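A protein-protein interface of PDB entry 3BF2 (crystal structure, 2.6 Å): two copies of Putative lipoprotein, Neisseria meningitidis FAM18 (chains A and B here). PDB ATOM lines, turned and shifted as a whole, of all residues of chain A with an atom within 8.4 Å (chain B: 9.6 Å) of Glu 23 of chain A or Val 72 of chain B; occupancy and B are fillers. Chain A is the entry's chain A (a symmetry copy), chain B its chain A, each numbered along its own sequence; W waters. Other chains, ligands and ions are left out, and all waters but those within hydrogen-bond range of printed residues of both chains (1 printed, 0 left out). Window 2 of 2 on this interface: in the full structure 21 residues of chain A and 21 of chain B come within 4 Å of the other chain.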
ATOM      1  N   TRP A  20       7.605  25.112 -25.103  1.00  0.00           N
ATOM      2  CA  TRP A  20       8.884  25.087 -24.380  1.00  0.00           C
ATOM      3  C   TRP A  20       9.263  23.891 -23.502  1.00  0.00           C
ATOM      4  O   TRP A  20       8.403  23.218 -22.932  1.00  0.00           O
ATOM      5  CB  TRP A  20       8.983  26.313 -23.485  1.00  0.00           C
ATOM      6  CG  TRP A  20       9.069  27.598 -24.212  1.00  0.00           C
ATOM      7  CD1 TRP A  20       8.036  28.328 -24.729  1.00  0.00           C
ATOM      8  CD2 TRP A  20      10.258  28.353 -24.457  1.00  0.00           C
ATOM      9  NE1 TRP A  20       8.513  29.501 -25.275  1.00  0.00           N
ATOM     10  CE2 TRP A  20       9.875  29.541 -25.117  1.00  0.00           C
ATOM     11  CE3 TRP A  20      11.614  28.145 -24.176  1.00  0.00           C
ATOM     12  CZ2 TRP A  20      10.791  30.513 -25.504  1.00  0.00           C
ATOM     13  CZ3 TRP A  20      12.528  29.112 -24.566  1.00  0.00           C
ATOM     14  CH2 TRP A  20      12.112  30.282 -25.218  1.00  0.00           C
ATOM     15  N   HIS A  21      10.570  23.653 -23.397  1.00  0.00           N
ATOM     16  CA  HIS A  21      11.134  22.616 -22.536  1.00  0.00           C
ATOM     17  C   HIS A  21      12.162  23.326 -21.652  1.00  0.00           C
ATOM     18  O   HIS A  21      12.951  24.145 -22.140  1.00  0.00           O
ATOM     19  CB  HIS A  21      11.849  21.534 -23.337  1.00  0.00           C
ATOM     20  CG  HIS A  21      12.577  20.555 -22.476  1.00  0.00           C
ATOM     21  ND1 HIS A  21      13.916  20.273 -22.628  1.00  0.00           N
ATOM     22  CD2 HIS A  21      12.164  19.861 -21.390  1.00  0.00           C
ATOM     23  CE1 HIS A  21      14.301  19.449 -21.666  1.00  0.00           C
ATOM     24  NE2 HIS A  21      13.256  19.185 -20.902  1.00  0.00           N
ATOM     25  N   ILE A  22      12.148  23.031 -20.358  1.00  0.00           N
ATOM     26  CA  ILE A  22      13.080  23.666 -19.436  1.00  0.00           C
ATOM     27  C   ILE A  22      14.141  22.687 -18.950  1.00  0.00           C
ATOM     28  O   ILE A  22      13.816  21.677 -18.330  1.00  0.00           O
ATOM     29  CB  ILE A  22      12.332  24.234 -18.199  1.00  0.00           C
ATOM     30  CG1 ILE A  22      11.241  25.201 -18.655  1.00  0.00           C
ATOM     31  CG2 ILE A  22      13.315  24.917 -17.250  1.00  0.00           C
ATOM     32  CD1 ILE A  22      10.343  25.696 -17.543  1.00  0.00           C
ATOM     33  N   GLU A  23      15.401  22.970 -19.254  1.00  0.00           N
ATOM     34  CA  GLU A  23      16.493  22.117 -18.805  1.00  0.00           C
ATOM     35  C   GLU A  23      17.157  22.759 -17.588  1.00  0.00           C
ATOM     36  O   GLU A  23      17.695  23.867 -17.673  1.00  0.00           O
ATOM     37  CB  GLU A  23      17.539  21.926 -19.918  1.00  0.00           C
ATOM     38  CG  GLU A  23      17.342  20.674 -20.762  1.00  0.00           C
ATOM     39  CD  GLU A  23      17.502  19.376 -19.964  1.00  0.00           C
ATOM     40  OE1 GLU A  23      18.611  19.121 -19.441  1.00  0.00           O
ATOM     41  OE2 GLU A  23      16.514  18.610 -19.862  1.00  0.00           O
ATOM     42  N   GLY A  24      17.107  22.065 -16.455  1.00  0.00           N
ATOM     43  CA  GLY A  24      17.719  22.578 -15.243  1.00  0.00           C
ATOM     44  C   GLY A  24      16.780  23.447 -14.434  1.00  0.00           C
ATOM     45  O   GLY A  24      15.566  23.411 -14.626  1.00  0.00           O
ATOM     46  N   GLY A  25      17.347  24.234 -13.528  1.00  0.00           N
ATOM     47  CA  GLY A  25      16.545  25.121 -12.709  1.00  0.00           C
ATOM     48  C   GLY A  25      15.362  24.424 -12.083  1.00  0.00           C
ATOM     49  O   GLY A  25      14.260  24.959 -12.089  1.00  0.00           O
ATOM     50  N   GLN A  26      15.591  23.235 -11.536  1.00  0.00           N
ATOM     51  CA  GLN A  26      14.529  22.462 -10.908  1.00  0.00           C
ATOM     52  C   GLN A  26      13.666  23.312  -9.968  1.00  0.00           C
ATOM     53  O   GLN A  26      12.440  23.279 -10.050  1.00  0.00           O
ATOM     54  CB  GLN A  26      15.121  21.286 -10.129  1.00  0.00           C
ATOM     55  CG  GLN A  26      15.982  20.317 -10.951  1.00  0.00           C
ATOM     56  CD  GLN A  26      17.340  20.894 -11.371  1.00  0.00           C
ATOM     57  OE1 GLN A  26      18.085  21.453 -10.554  1.00  0.00           O
ATOM     58  NE2 GLN A  26      17.672  20.742 -12.654  1.00  0.00           N
ATOM     59  N   GLN A  29      11.468  25.510 -11.968  1.00  0.00           N
ATOM     60  CA  GLN A  29      10.596  24.852 -12.916  1.00  0.00           C
ATOM     61  C   GLN A  29       9.088  25.148 -12.792  1.00  0.00           C
ATOM     62  O   GLN A  29       8.456  25.519 -13.784  1.00  0.00           O
ATOM     63  CB  GLN A  29      10.862  23.347 -12.871  1.00  0.00           C
ATOM     64  CG  GLN A  29      10.681  22.690 -14.213  1.00  0.00           C
ATOM     65  CD  GLN A  29      11.838  21.784 -14.578  1.00  0.00           C
ATOM     66  OE1 GLN A  29      13.010  22.183 -14.546  1.00  0.00           O
ATOM     67  NE2 GLN A  29      11.514  20.550 -14.934  1.00  0.00           N
ATOM     68  N   LEU A  32       8.103  28.971 -13.407  1.00  0.00           N
ATOM     69  CA  LEU A  32       8.327  29.260 -14.821  1.00  0.00           C
ATOM     70  C   LEU A  32       7.182  28.687 -15.643  1.00  0.00           C
ATOM     71  O   LEU A  32       6.594  29.390 -16.465  1.00  0.00           O
ATOM     72  CB  LEU A  32       9.639  28.642 -15.296  1.00  0.00           C
ATOM     73  CG  LEU A  32      10.933  29.411 -15.039  1.00  0.00           C
ATOM     74  CD1 LEU A  32      12.127  28.524 -15.420  1.00  0.00           C
ATOM     75  CD2 LEU A  32      10.916  30.712 -15.858  1.00  0.00           C
ATOM     76  N   ASP A  44       6.607  21.099 -22.660  1.00  0.00           N
ATOM     77  CA  ASP A  44       6.634  19.733 -23.166  1.00  0.00           C
ATOM     78  C   ASP A  44       7.993  19.080 -22.945  1.00  0.00           C
ATOM     79  O   ASP A  44       8.905  19.693 -22.387  1.00  0.00           O
ATOM     80  CB  ASP A  44       6.307  19.753 -24.662  1.00  0.00           C
ATOM     81  CG  ASP A  44       5.594  18.499 -25.130  1.00  0.00           C
ATOM     82  OD1 ASP A  44       4.446  18.612 -25.629  1.00  0.00           O
ATOM     83  OD2 ASP A  44       6.175  17.402 -24.995  1.00  0.00           O
ATOM     84  N   ASP A  45       8.115  17.830 -23.384  1.00  0.00           N
ATOM     85  CA  ASP A  45       9.362  17.087 -23.259  1.00  0.00           C
ATOM     86  C   ASP A  45      10.340  17.729 -24.230  1.00  0.00           C
ATOM     87  O   ASP A  45       9.942  18.534 -25.074  1.00  0.00           O
ATOM     88  CB  ASP A  45       9.139  15.612 -23.621  1.00  0.00           C
ATOM     89  N   ALA A  46      11.615  17.375 -24.121  1.00  0.00           N
ATOM     90  CA  ALA A  46      12.616  17.944 -25.012  1.00  0.00           C
ATOM     91  C   ALA A  46      12.210  17.647 -26.452  1.00  0.00           C
ATOM     92  O   ALA A  46      12.213  18.533 -27.319  1.00  0.00           O
ATOM     93  CB  ALA A  46      13.987  17.341 -24.719  1.00  0.00           C
ATOM     94  N   MET A  51      11.062  25.097 -28.553  1.00  0.00           N
ATOM     95  CA  MET A  51      12.031  25.849 -27.765  1.00  0.00           C
ATOM     96  C   MET A  51      12.545  25.167 -26.497  1.00  0.00           C
ATOM     97  O   MET A  51      11.874  24.321 -25.902  1.00  0.00           O
ATOM     98  CB  MET A  51      11.407  27.178 -27.378  1.00  0.00           C
ATOM     99  CG  MET A  51      12.036  28.368 -28.045  1.00  0.00           C
ATOM    100  SD  MET A  51      11.882  28.384 -29.972  1.00  0.00           S
ATOM    101  CE  MET A  51      12.430  30.221 -30.186  1.00  0.00           C
ATOM    102  N   THR A  52      13.749  25.555 -26.094  1.00  0.00           N
ATOM    103  CA  THR A  52      14.362  25.043 -24.883  1.00  0.00           C
ATOM    104  C   THR A  52      14.981  26.203 -24.112  1.00  0.00           C
ATOM    105  O   THR A  52      15.681  27.044 -24.675  1.00  0.00           O
ATOM    106  CB  THR A  52      15.444  23.989 -25.179  1.00  0.00           C
ATOM    107  OG1 THR A  52      14.815  22.804 -25.679  1.00  0.00           O
ATOM    108  CG2 THR A  52      16.212  23.629 -23.911  1.00  0.00           C
ATOM    109  N   LEU A  53      14.679  26.258 -22.824  1.00  0.00           N
ATOM    110  CA  LEU A  53      15.208  27.285 -21.952  1.00  0.00           C
ATOM    111  C   LEU A  53      16.148  26.531 -21.035  1.00  0.00           C
ATOM    112  O   LEU A  53      15.705  25.748 -20.200  1.00  0.00           O
ATOM    113  CB  LEU A  53      14.076  27.933 -21.148  1.00  0.00           C
ATOM    114  CG  LEU A  53      14.498  28.973 -20.109  1.00  0.00           C
ATOM    115  CD1 LEU A  53      15.202  30.131 -20.798  1.00  0.00           C
ATOM    116  CD2 LEU A  53      13.265  29.453 -19.358  1.00  0.00           C
ATOM    117  N   ARG A  54      17.445  26.749 -21.207  1.00  0.00           N
ATOM    118  CA  ARG A  54      18.435  26.051 -20.398  1.00  0.00           C
ATOM    119  C   ARG A  54      18.981  26.911 -19.263  1.00  0.00           C
ATOM    120  O   ARG A  54      19.649  27.927 -19.500  1.00  0.00           O
ATOM    121  CB  ARG A  54      19.588  25.585 -21.281  1.00  0.00           C
ATOM    122  CG  ARG A  54      20.545  24.621 -20.618  1.00  0.00           C
ATOM    123  CD  ARG A  54      21.715  24.359 -21.542  1.00  0.00           C
ATOM    124  NE  ARG A  54      22.506  25.572 -21.724  1.00  0.00           N
ATOM    125  CZ  ARG A  54      23.155  25.887 -22.840  1.00  0.00           C
ATOM    126  NH1 ARG A  54      23.113  25.079 -23.895  1.00  0.00           N
ATOM    127  NH2 ARG A  54      23.850  27.018 -22.901  1.00  0.00           N
ATOM    128  N   ILE A  55      18.681  26.507 -18.034  1.00  0.00           N
ATOM    129  CA  ILE A  55      19.161  27.209 -16.855  1.00  0.00           C
ATOM    130  C   ILE A  55      20.617  26.770 -16.653  1.00  0.00           C
ATOM    131  O   ILE A  55      20.884  25.613 -16.341  1.00  0.00           O
ATOM    132  CB  ILE A  55      18.349  26.816 -15.612  1.00  0.00           C
ATOM    133  CG1 ILE A  55      16.859  27.088 -15.859  1.00  0.00           C
ATOM    134  CG2 ILE A  55      18.849  27.601 -14.398  1.00  0.00           C
ATOM    135  CD1 ILE A  55      16.524  28.555 -16.062  1.00  0.00           C
ATOM    136  N   ASP A  56      21.555  27.690 -16.837  1.00  0.00           N
ATOM    137  CA  ASP A  56      22.955  27.355 -16.678  1.00  0.00           C
ATOM    138  C   ASP A  56      23.464  27.575 -15.273  1.00  0.00           C
ATOM    139  O   ASP A  56      24.420  26.929 -14.847  1.00  0.00           O
ATOM    140  CB  ASP A  56      23.816  28.159 -17.648  1.00  0.00           C
ATOM    141  CG  ASP A  56      23.515  27.834 -19.094  1.00  0.00           C
ATOM    142  OD1 ASP A  56      23.406  26.631 -19.437  1.00  0.00           O
ATOM    143  OD2 ASP A  56      23.394  28.788 -19.891  1.00  0.00           O
ATOM    144  N   SER A  57      22.830  28.483 -14.549  1.00  0.00           N
ATOM    145  CA  SER A  57      23.266  28.762 -13.199  1.00  0.00           C
ATOM    146  C   SER A  57      22.200  29.402 -12.333  1.00  0.00           C
ATOM    147  O   SER A  57      21.430  30.244 -12.797  1.00  0.00           O
ATOM    148  CB  SER A  57      24.491  29.671 -13.226  1.00  0.00           C
ATOM    149  OG  SER A  57      24.649  30.312 -11.967  1.00  0.00           O
ATOM    150  N   VAL A  58      22.165  28.997 -11.071  1.00  0.00           N
ATOM    151  CA  VAL A  58      21.223  29.567 -10.118  1.00  0.00           C
ATOM    152  C   VAL A  58      22.045  29.860  -8.883  1.00  0.00           C
ATOM    153  O   VAL A  58      22.741  28.997  -8.368  1.00  0.00           O
ATOM    154  CB  VAL A  58      20.085  28.599  -9.771  1.00  0.00           C
ATOM    155  CG1 VAL A  58      19.167  29.240  -8.733  1.00  0.00           C
ATOM    156  CG2 VAL A  58      19.291  28.270 -11.024  1.00  0.00           C
ATOM    157  N   GLU A  83      20.885  32.456 -14.606  1.00  0.00           N
ATOM    158  CA  GLU A  83      21.453  32.622 -15.935  1.00  0.00           C
ATOM    159  C   GLU A  83      20.852  31.540 -16.811  1.00  0.00           C
ATOM    160  O   GLU A  83      20.856  30.359 -16.459  1.00  0.00           O
ATOM    161  CB  GLU A  83      22.972  32.470 -15.894  1.00  0.00           C
ATOM    162  CG  GLU A  83      23.698  33.698 -15.355  1.00  0.00           C
ATOM    163  CD  GLU A  83      25.079  33.371 -14.792  1.00  0.00           C
ATOM    164  OE1 GLU A  83      25.729  32.420 -15.297  1.00  0.00           O
ATOM    165  OE2 GLU A  83      25.517  34.077 -13.851  1.00  0.00           O
ATOM    166  N   ALA A  84      20.315  31.939 -17.953  1.00  0.00           N
ATOM    167  CA  ALA A  84      19.707  30.977 -18.842  1.00  0.00           C
ATOM    168  C   ALA A  84      20.001  31.295 -20.304  1.00  0.00           C
ATOM    169  O   ALA A  84      20.292  32.434 -20.675  1.00  0.00           O
ATOM    170  CB  ALA A  84      18.205  30.942 -18.596  1.00  0.00           C
ATOM    171  N   GLN A  85      19.920  30.264 -21.127  1.00  0.00           N
ATOM    172  CA  GLN A  85      20.163  30.395 -22.548  1.00  0.00           C
ATOM    173  C   GLN A  85      18.945  29.831 -23.275  1.00  0.00           C
ATOM    174  O   GLN A  85      18.418  28.779 -22.908  1.00  0.00           O
ATOM    175  CB  GLN A  85      21.425  29.606 -22.930  1.00  0.00           C
ATOM    176  CG  GLN A  85      21.735  29.596 -24.416  1.00  0.00           C
ATOM    177  CD  GLN A  85      22.053  30.980 -24.949  1.00  0.00           C
ATOM    178  OE1 GLN A  85      23.010  31.618 -24.501  1.00  0.00           O
ATOM    179  NE2 GLN A  85      21.256  31.451 -25.911  1.00  0.00           N
ATOM    180  N   LEU A  87      17.368  28.220 -26.620  1.00  0.00           N
ATOM    181  CA  LEU A  87      17.862  27.410 -27.729  1.00  0.00           C
ATOM    182  C   LEU A  87      16.728  27.018 -28.660  1.00  0.00           C
ATOM    183  O   LEU A  87      15.628  26.712 -28.205  1.00  0.00           O
ATOM    184  CB  LEU A  87      18.520  26.132 -27.199  1.00  0.00           C
ATOM    185  CG  LEU A  87      19.817  26.243 -26.393  1.00  0.00           C
ATOM    186  CD1 LEU A  87      19.877  25.103 -25.401  1.00  0.00           C
ATOM    187  CD2 LEU A  87      21.026  26.208 -27.329  1.00  0.00           C
ATOM    188  N   GLY A  90      18.373  22.847 -30.759  1.00  0.00           N
ATOM    189  CA  GLY A  90      19.801  22.677 -30.566  1.00  0.00           C
ATOM    190  C   GLY A  90      20.681  23.906 -30.739  1.00  0.00           C
ATOM    191  O   GLY A  90      21.820  23.917 -30.259  1.00  0.00           O
ATOM    192  N   LYS B  62      24.571  26.923  -7.821  1.00  0.00           N
ATOM    193  CA  LYS B  62      24.340  25.688  -8.569  1.00  0.00           C
ATOM    194  C   LYS B  62      24.676  26.005 -10.022  1.00  0.00           C
ATOM    195  O   LYS B  62      24.042  26.857 -10.651  1.00  0.00           O
ATOM    196  CB  LYS B  62      22.881  25.249  -8.453  1.00  0.00           C
ATOM    197  CG  LYS B  62      22.597  23.896  -9.102  1.00  0.00           C
ATOM    198  CD  LYS B  62      21.144  23.491  -8.942  1.00  0.00           C
ATOM    199  CE  LYS B  62      20.229  24.407  -9.746  1.00  0.00           C
ATOM    200  NZ  LYS B  62      18.820  24.373  -9.249  1.00  0.00           N
ATOM    201  N   THR B  64      25.767  24.551 -14.050  1.00  0.00           N
ATOM    202  CA  THR B  64      25.666  23.460 -15.000  1.00  0.00           C
ATOM    203  C   THR B  64      27.086  22.968 -15.213  1.00  0.00           C
ATOM    204  O   THR B  64      28.006  23.752 -15.459  1.00  0.00           O
ATOM    205  CB  THR B  64      25.015  23.930 -16.319  1.00  0.00           C
ATOM    206  OG1 THR B  64      23.775  23.228 -16.497  1.00  0.00           O
ATOM    207  CG2 THR B  64      25.927  23.670 -17.525  1.00  0.00           C
ATOM    208  N   TYR B  65      27.267  21.660 -15.091  1.00  0.00           N
ATOM    209  CA  TYR B  65      28.592  21.057 -15.223  1.00  0.00           C
ATOM    210  C   TYR B  65      28.749  20.294 -16.531  1.00  0.00           C
ATOM    211  O   TYR B  65      29.289  20.826 -17.493  1.00  0.00           O
ATOM    212  CB  TYR B  65      28.829  20.147 -14.020  1.00  0.00           C
ATOM    213  CG  TYR B  65      30.231  19.616 -13.880  1.00  0.00           C
ATOM    214  CD1 TYR B  65      31.338  20.444 -14.088  1.00  0.00           C
ATOM    215  CD2 TYR B  65      30.458  18.293 -13.498  1.00  0.00           C
ATOM    216  CE1 TYR B  65      32.635  19.969 -13.919  1.00  0.00           C
ATOM    217  CE2 TYR B  65      31.749  17.807 -13.321  1.00  0.00           C
ATOM    218  CZ  TYR B  65      32.832  18.651 -13.535  1.00  0.00           C
ATOM    219  OH  TYR B  65      34.110  18.173 -13.360  1.00  0.00           O
ATOM    220  N   THR B  66      28.288  19.050 -16.562  1.00  0.00           N
ATOM    221  CA  THR B  66      28.358  18.244 -17.778  1.00  0.00           C
ATOM    222  C   THR B  66      27.140  18.641 -18.604  1.00  0.00           C
ATOM    223  O   THR B  66      26.001  18.557 -18.129  1.00  0.00           O
ATOM    224  CB  THR B  66      28.247  16.728 -17.473  1.00  0.00           C
ATOM    225  OG1 THR B  66      28.945  16.429 -16.258  1.00  0.00           O
ATOM    226  CG2 THR B  66      28.839  15.907 -18.610  1.00  0.00           C
ATOM    227  N   VAL B  67      27.364  19.086 -19.833  1.00  0.00           N
ATOM    228  CA  VAL B  67      26.238  19.466 -20.671  1.00  0.00           C
ATOM    229  C   VAL B  67      25.805  18.264 -21.494  1.00  0.00           C
ATOM    230  O   VAL B  67      24.777  17.644 -21.213  1.00  0.00           O
ATOM    231  CB  VAL B  67      26.594  20.629 -21.625  1.00  0.00           C
ATOM    232  CG1 VAL B  67      25.499  20.791 -22.680  1.00  0.00           C
ATOM    233  CG2 VAL B  67      26.741  21.918 -20.834  1.00  0.00           C
ATOM    234  N   THR B  68      26.612  17.934 -22.500  1.00  0.00           N
ATOM    235  CA  THR B  68      26.348  16.805 -23.386  1.00  0.00           C
ATOM    236  C   THR B  68      25.309  17.148 -24.442  1.00  0.00           C
ATOM    237  O   THR B  68      25.611  17.170 -25.637  1.00  0.00           O
ATOM    238  CB  THR B  68      25.887  15.595 -22.576  1.00  0.00           C
ATOM    239  N   ALA B  71      22.761  20.767 -24.965  1.00  0.00           N
ATOM    240  CA  ALA B  71      21.484  21.379 -24.597  1.00  0.00           C
ATOM    241  C   ALA B  71      20.701  20.494 -23.627  1.00  0.00           C
ATOM    242  O   ALA B  71      19.484  20.640 -23.483  1.00  0.00           O
ATOM    243  CB  ALA B  71      20.650  21.635 -25.844  1.00  0.00           C
ATOM    244  N   VAL B  72      21.402  19.581 -22.963  1.00  0.00           N
ATOM    245  CA  VAL B  72      20.767  18.670 -22.017  1.00  0.00           C
ATOM    246  C   VAL B  72      21.700  18.383 -20.845  1.00  0.00           C
ATOM    247  O   VAL B  72      22.470  17.420 -20.881  1.00  0.00           O
ATOM    248  CB  VAL B  72      20.396  17.367 -22.732  1.00  0.00           C
ATOM    249  N   ILE B  73      21.623  19.219 -19.813  1.00  0.00           N
ATOM    250  CA  ILE B  73      22.460  19.070 -18.629  1.00  0.00           C
ATOM    251  C   ILE B  73      22.348  17.680 -18.008  1.00  0.00           C
ATOM    252  O   ILE B  73      21.250  17.151 -17.803  1.00  0.00           O
ATOM    253  CB  ILE B  73      22.094  20.135 -17.593  1.00  0.00           C
ATOM    254  N   ASN B  74      23.497  17.085 -17.724  1.00  0.00           N
ATOM    255  CA  ASN B  74      23.537  15.770 -17.115  1.00  0.00           C
ATOM    256  C   ASN B  74      23.943  15.929 -15.649  1.00  0.00           C
ATOM    257  O   ASN B  74      23.386  15.272 -14.764  1.00  0.00           O
ATOM    258  CB  ASN B  74      24.531  14.883 -17.865  1.00  0.00           C
ATOM    259  N   GLU B  75      24.899  16.824 -15.392  1.00  0.00           N
ATOM    260  CA  GLU B  75      25.366  17.072 -14.030  1.00  0.00           C
ATOM    261  C   GLU B  75      25.551  18.546 -13.662  1.00  0.00           C
ATOM    262  O   GLU B  75      25.836  19.400 -14.508  1.00  0.00           O
ATOM    263  CB  GLU B  75      26.688  16.354 -13.785  1.00  0.00           C
ATOM    264  CG  GLU B  75      26.682  14.874 -14.058  1.00  0.00           C
ATOM    265  CD  GLU B  75      28.026  14.267 -13.735  1.00  0.00           C
ATOM    266  OE1 GLU B  75      29.037  14.759 -14.289  1.00  0.00           O
ATOM    267  OE2 GLU B  75      28.077  13.316 -12.923  1.00  0.00           O
ATOM    268  N   TYR B  76      25.417  18.814 -12.369  1.00  0.00           N
ATOM    269  CA  TYR B  76      25.567  20.157 -11.828  1.00  0.00           C
ATOM    270  C   TYR B  76      26.687  20.207 -10.795  1.00  0.00           C
ATOM    271  O   TYR B  76      26.963  19.228 -10.093  1.00  0.00           O
ATOM    272  CB  TYR B  76      24.275  20.597 -11.135  1.00  0.00           C
ATOM    273  CG  TYR B  76      23.052  20.561 -12.003  1.00  0.00           C
ATOM    274  CD1 TYR B  76      22.683  21.667 -12.771  1.00  0.00           C
ATOM    275  CD2 TYR B  76      22.251  19.417 -12.050  1.00  0.00           C
ATOM    276  CE1 TYR B  76      21.543  21.638 -13.561  1.00  0.00           C
ATOM    277  CE2 TYR B  76      21.113  19.370 -12.834  1.00  0.00           C
ATOM    278  CZ  TYR B  76      20.760  20.481 -13.588  1.00  0.00           C
ATOM    279  OH  TYR B  76      19.626  20.414 -14.368  1.00  0.00           O
ATOM    280  N   TYR B 107      21.234  13.056 -10.563  1.00  0.00           N
ATOM    281  CA  TYR B 107      20.017  12.341 -10.151  1.00  0.00           C
ATOM    282  C   TYR B 107      19.867  10.997 -10.862  1.00  0.00           C
ATOM    283  O   TYR B 107      20.347  10.815 -11.979  1.00  0.00           O
ATOM    284  CB  TYR B 107      18.764  13.154 -10.479  1.00  0.00           C
ATOM    285  CG  TYR B 107      18.843  14.636 -10.247  1.00  0.00           C
ATOM    286  CD1 TYR B 107      18.705  15.176  -8.966  1.00  0.00           C
ATOM    287  CD2 TYR B 107      18.984  15.511 -11.322  1.00  0.00           C
ATOM    288  CE1 TYR B 107      18.697  16.558  -8.764  1.00  0.00           C
ATOM    289  CE2 TYR B 107      18.982  16.892 -11.136  1.00  0.00           C
ATOM    290  CZ  TYR B 107      18.833  17.410  -9.858  1.00  0.00           C
ATOM    291  OH  TYR B 107      18.808  18.773  -9.677  1.00  0.00           O
HETATM  292  O   HOH W   1      18.193  18.188 -14.152  1.00  0.00           O
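The side-chain amino group (NZ) of Lys 62 of chain B sits at hydrogen-bond distance from the side-chain amide oxygen (OE1) of Gln 26 of chain A (3.3 Å).
O of Val 58 of chain A is in hydrogen-bond range of N of Lys 62 of chain B.
N of Thr 64 of chain B lies within hydrogen-bond range of O of Asp 56 of chain A (2.8 Å).
N of Ile 73 of chain B lies within hydrogen-bond range of OE1 of Glu 23 of chain A, 3.0 Å away.
The side-chain amide nitrogen of Gln 26 of chain A lies within hydrogen-bond range of the side-chain hydroxyl of Tyr 76 of chain B.
OH of Tyr 107 of chain B lies within hydrogen-bond range of OE1 of Gln 26 of chain A, at 2.9 Å.
NE2 of His 21 of chain A sits close to OE2 of Glu 23 of chain A (3.5 Å).
The backbone carbonyl oxygen (O) of Glu 23 of chain A sits at hydrogen-bond distance from the backbone NH (N) of Ile 55 of chain A (2.8 Å).
The backbone carbonyl oxygen (O) of Gly 24 of chain A sits close to the side-chain amide oxygen (OE1) of Gln 29 of chain A (2.8 Å).
The backbone carbonyl oxygen of Thr 52 of chain A lies within hydrogen-bond range of the backbone NH of Leu 87 of chain A (2.8 Å).
NE of Arg 54 of chain A is in salt-bridge range of OD1 of Asp 56 of chain A.
The backbone NH (N) of Asp 56 of chain A lies within hydrogen-bond range of the backbone carbonyl oxygen (O) of Glu 83 of chain A, 2.8 Å away.
CG of Glu 23 of chain A touches O of Ala 71 of chain B, 3.5 Å away.
Glu 23 of chain A touches Val 72 of chain B.
Gly 24 of chain A touches Tyr 76 of chain B.
Ile 55 of chain A touches Thr 64 of chain B (O to OG1, 3.8 Å).
CA of Ser 57 of chain A touches O of Lys 62 of chain B, 3.3 Å away.
Ala 71 of chain B touches Leu 87 of chain A (CB to CD1, 3.6 Å).
Of chain A, only Glu 23 (3.4 Å) comes within 4 Å of Val 72 of chain B.
Gly 24 of chain A touches just one residue of chain B: Tyr 76.
Ile 55 of chain A touches just one residue of chain B: Thr 64 (3.8 Å).
Ala 71 of chain B touches just these residues of chain A: Glu 23 and Leu 87.
Of the printed residues of chain A, Tyr 107 of chain B touches Gln 26.
Printed residues of chain B within 4 Å of Gln 26 of chain A: Lys 62 (3.3 Å), Tyr 76 (2.6 Å) and Tyr 107 (2.9 Å).
Printed residues of chain B within 4 Å of Leu 87 of chain A: Ala 71 (3.6 Å).
Leu 32 of chain A touches none of the printed residues of chain B.
The nearest residue of chain A that does not touch Val 72 of chain B is Arg 54 of chain A (5.0 Å).
The nearest printed residue of chain B that does not touch Gln 26 of chain A is Ile 73 of chain B (6.7 Å).
Printed residues of chain A that touch a printed residue of chain B: Glu 23, Gly 24, Gln 26, Ile 55, Asp 56, Ser 57, Val 58 and Leu 87.
Hydrophobic or aromatic side chains of chain A within 4 Å of the printed part of chain B: Leu 87.
Among the printed residues, 12 pairs touch across the chains.
Among the printed residues, no Asp or Glu carboxylate lies within 4 Å of a Lys or Arg side-chain nitrogen of the other chain.
No position is printed for both chains.
Water W1 lies within hydrogen-bond range of OH of Tyr 76 of chain B (2.7 Å) and NE2 of Gln 26 of chain A (3.0 Å).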
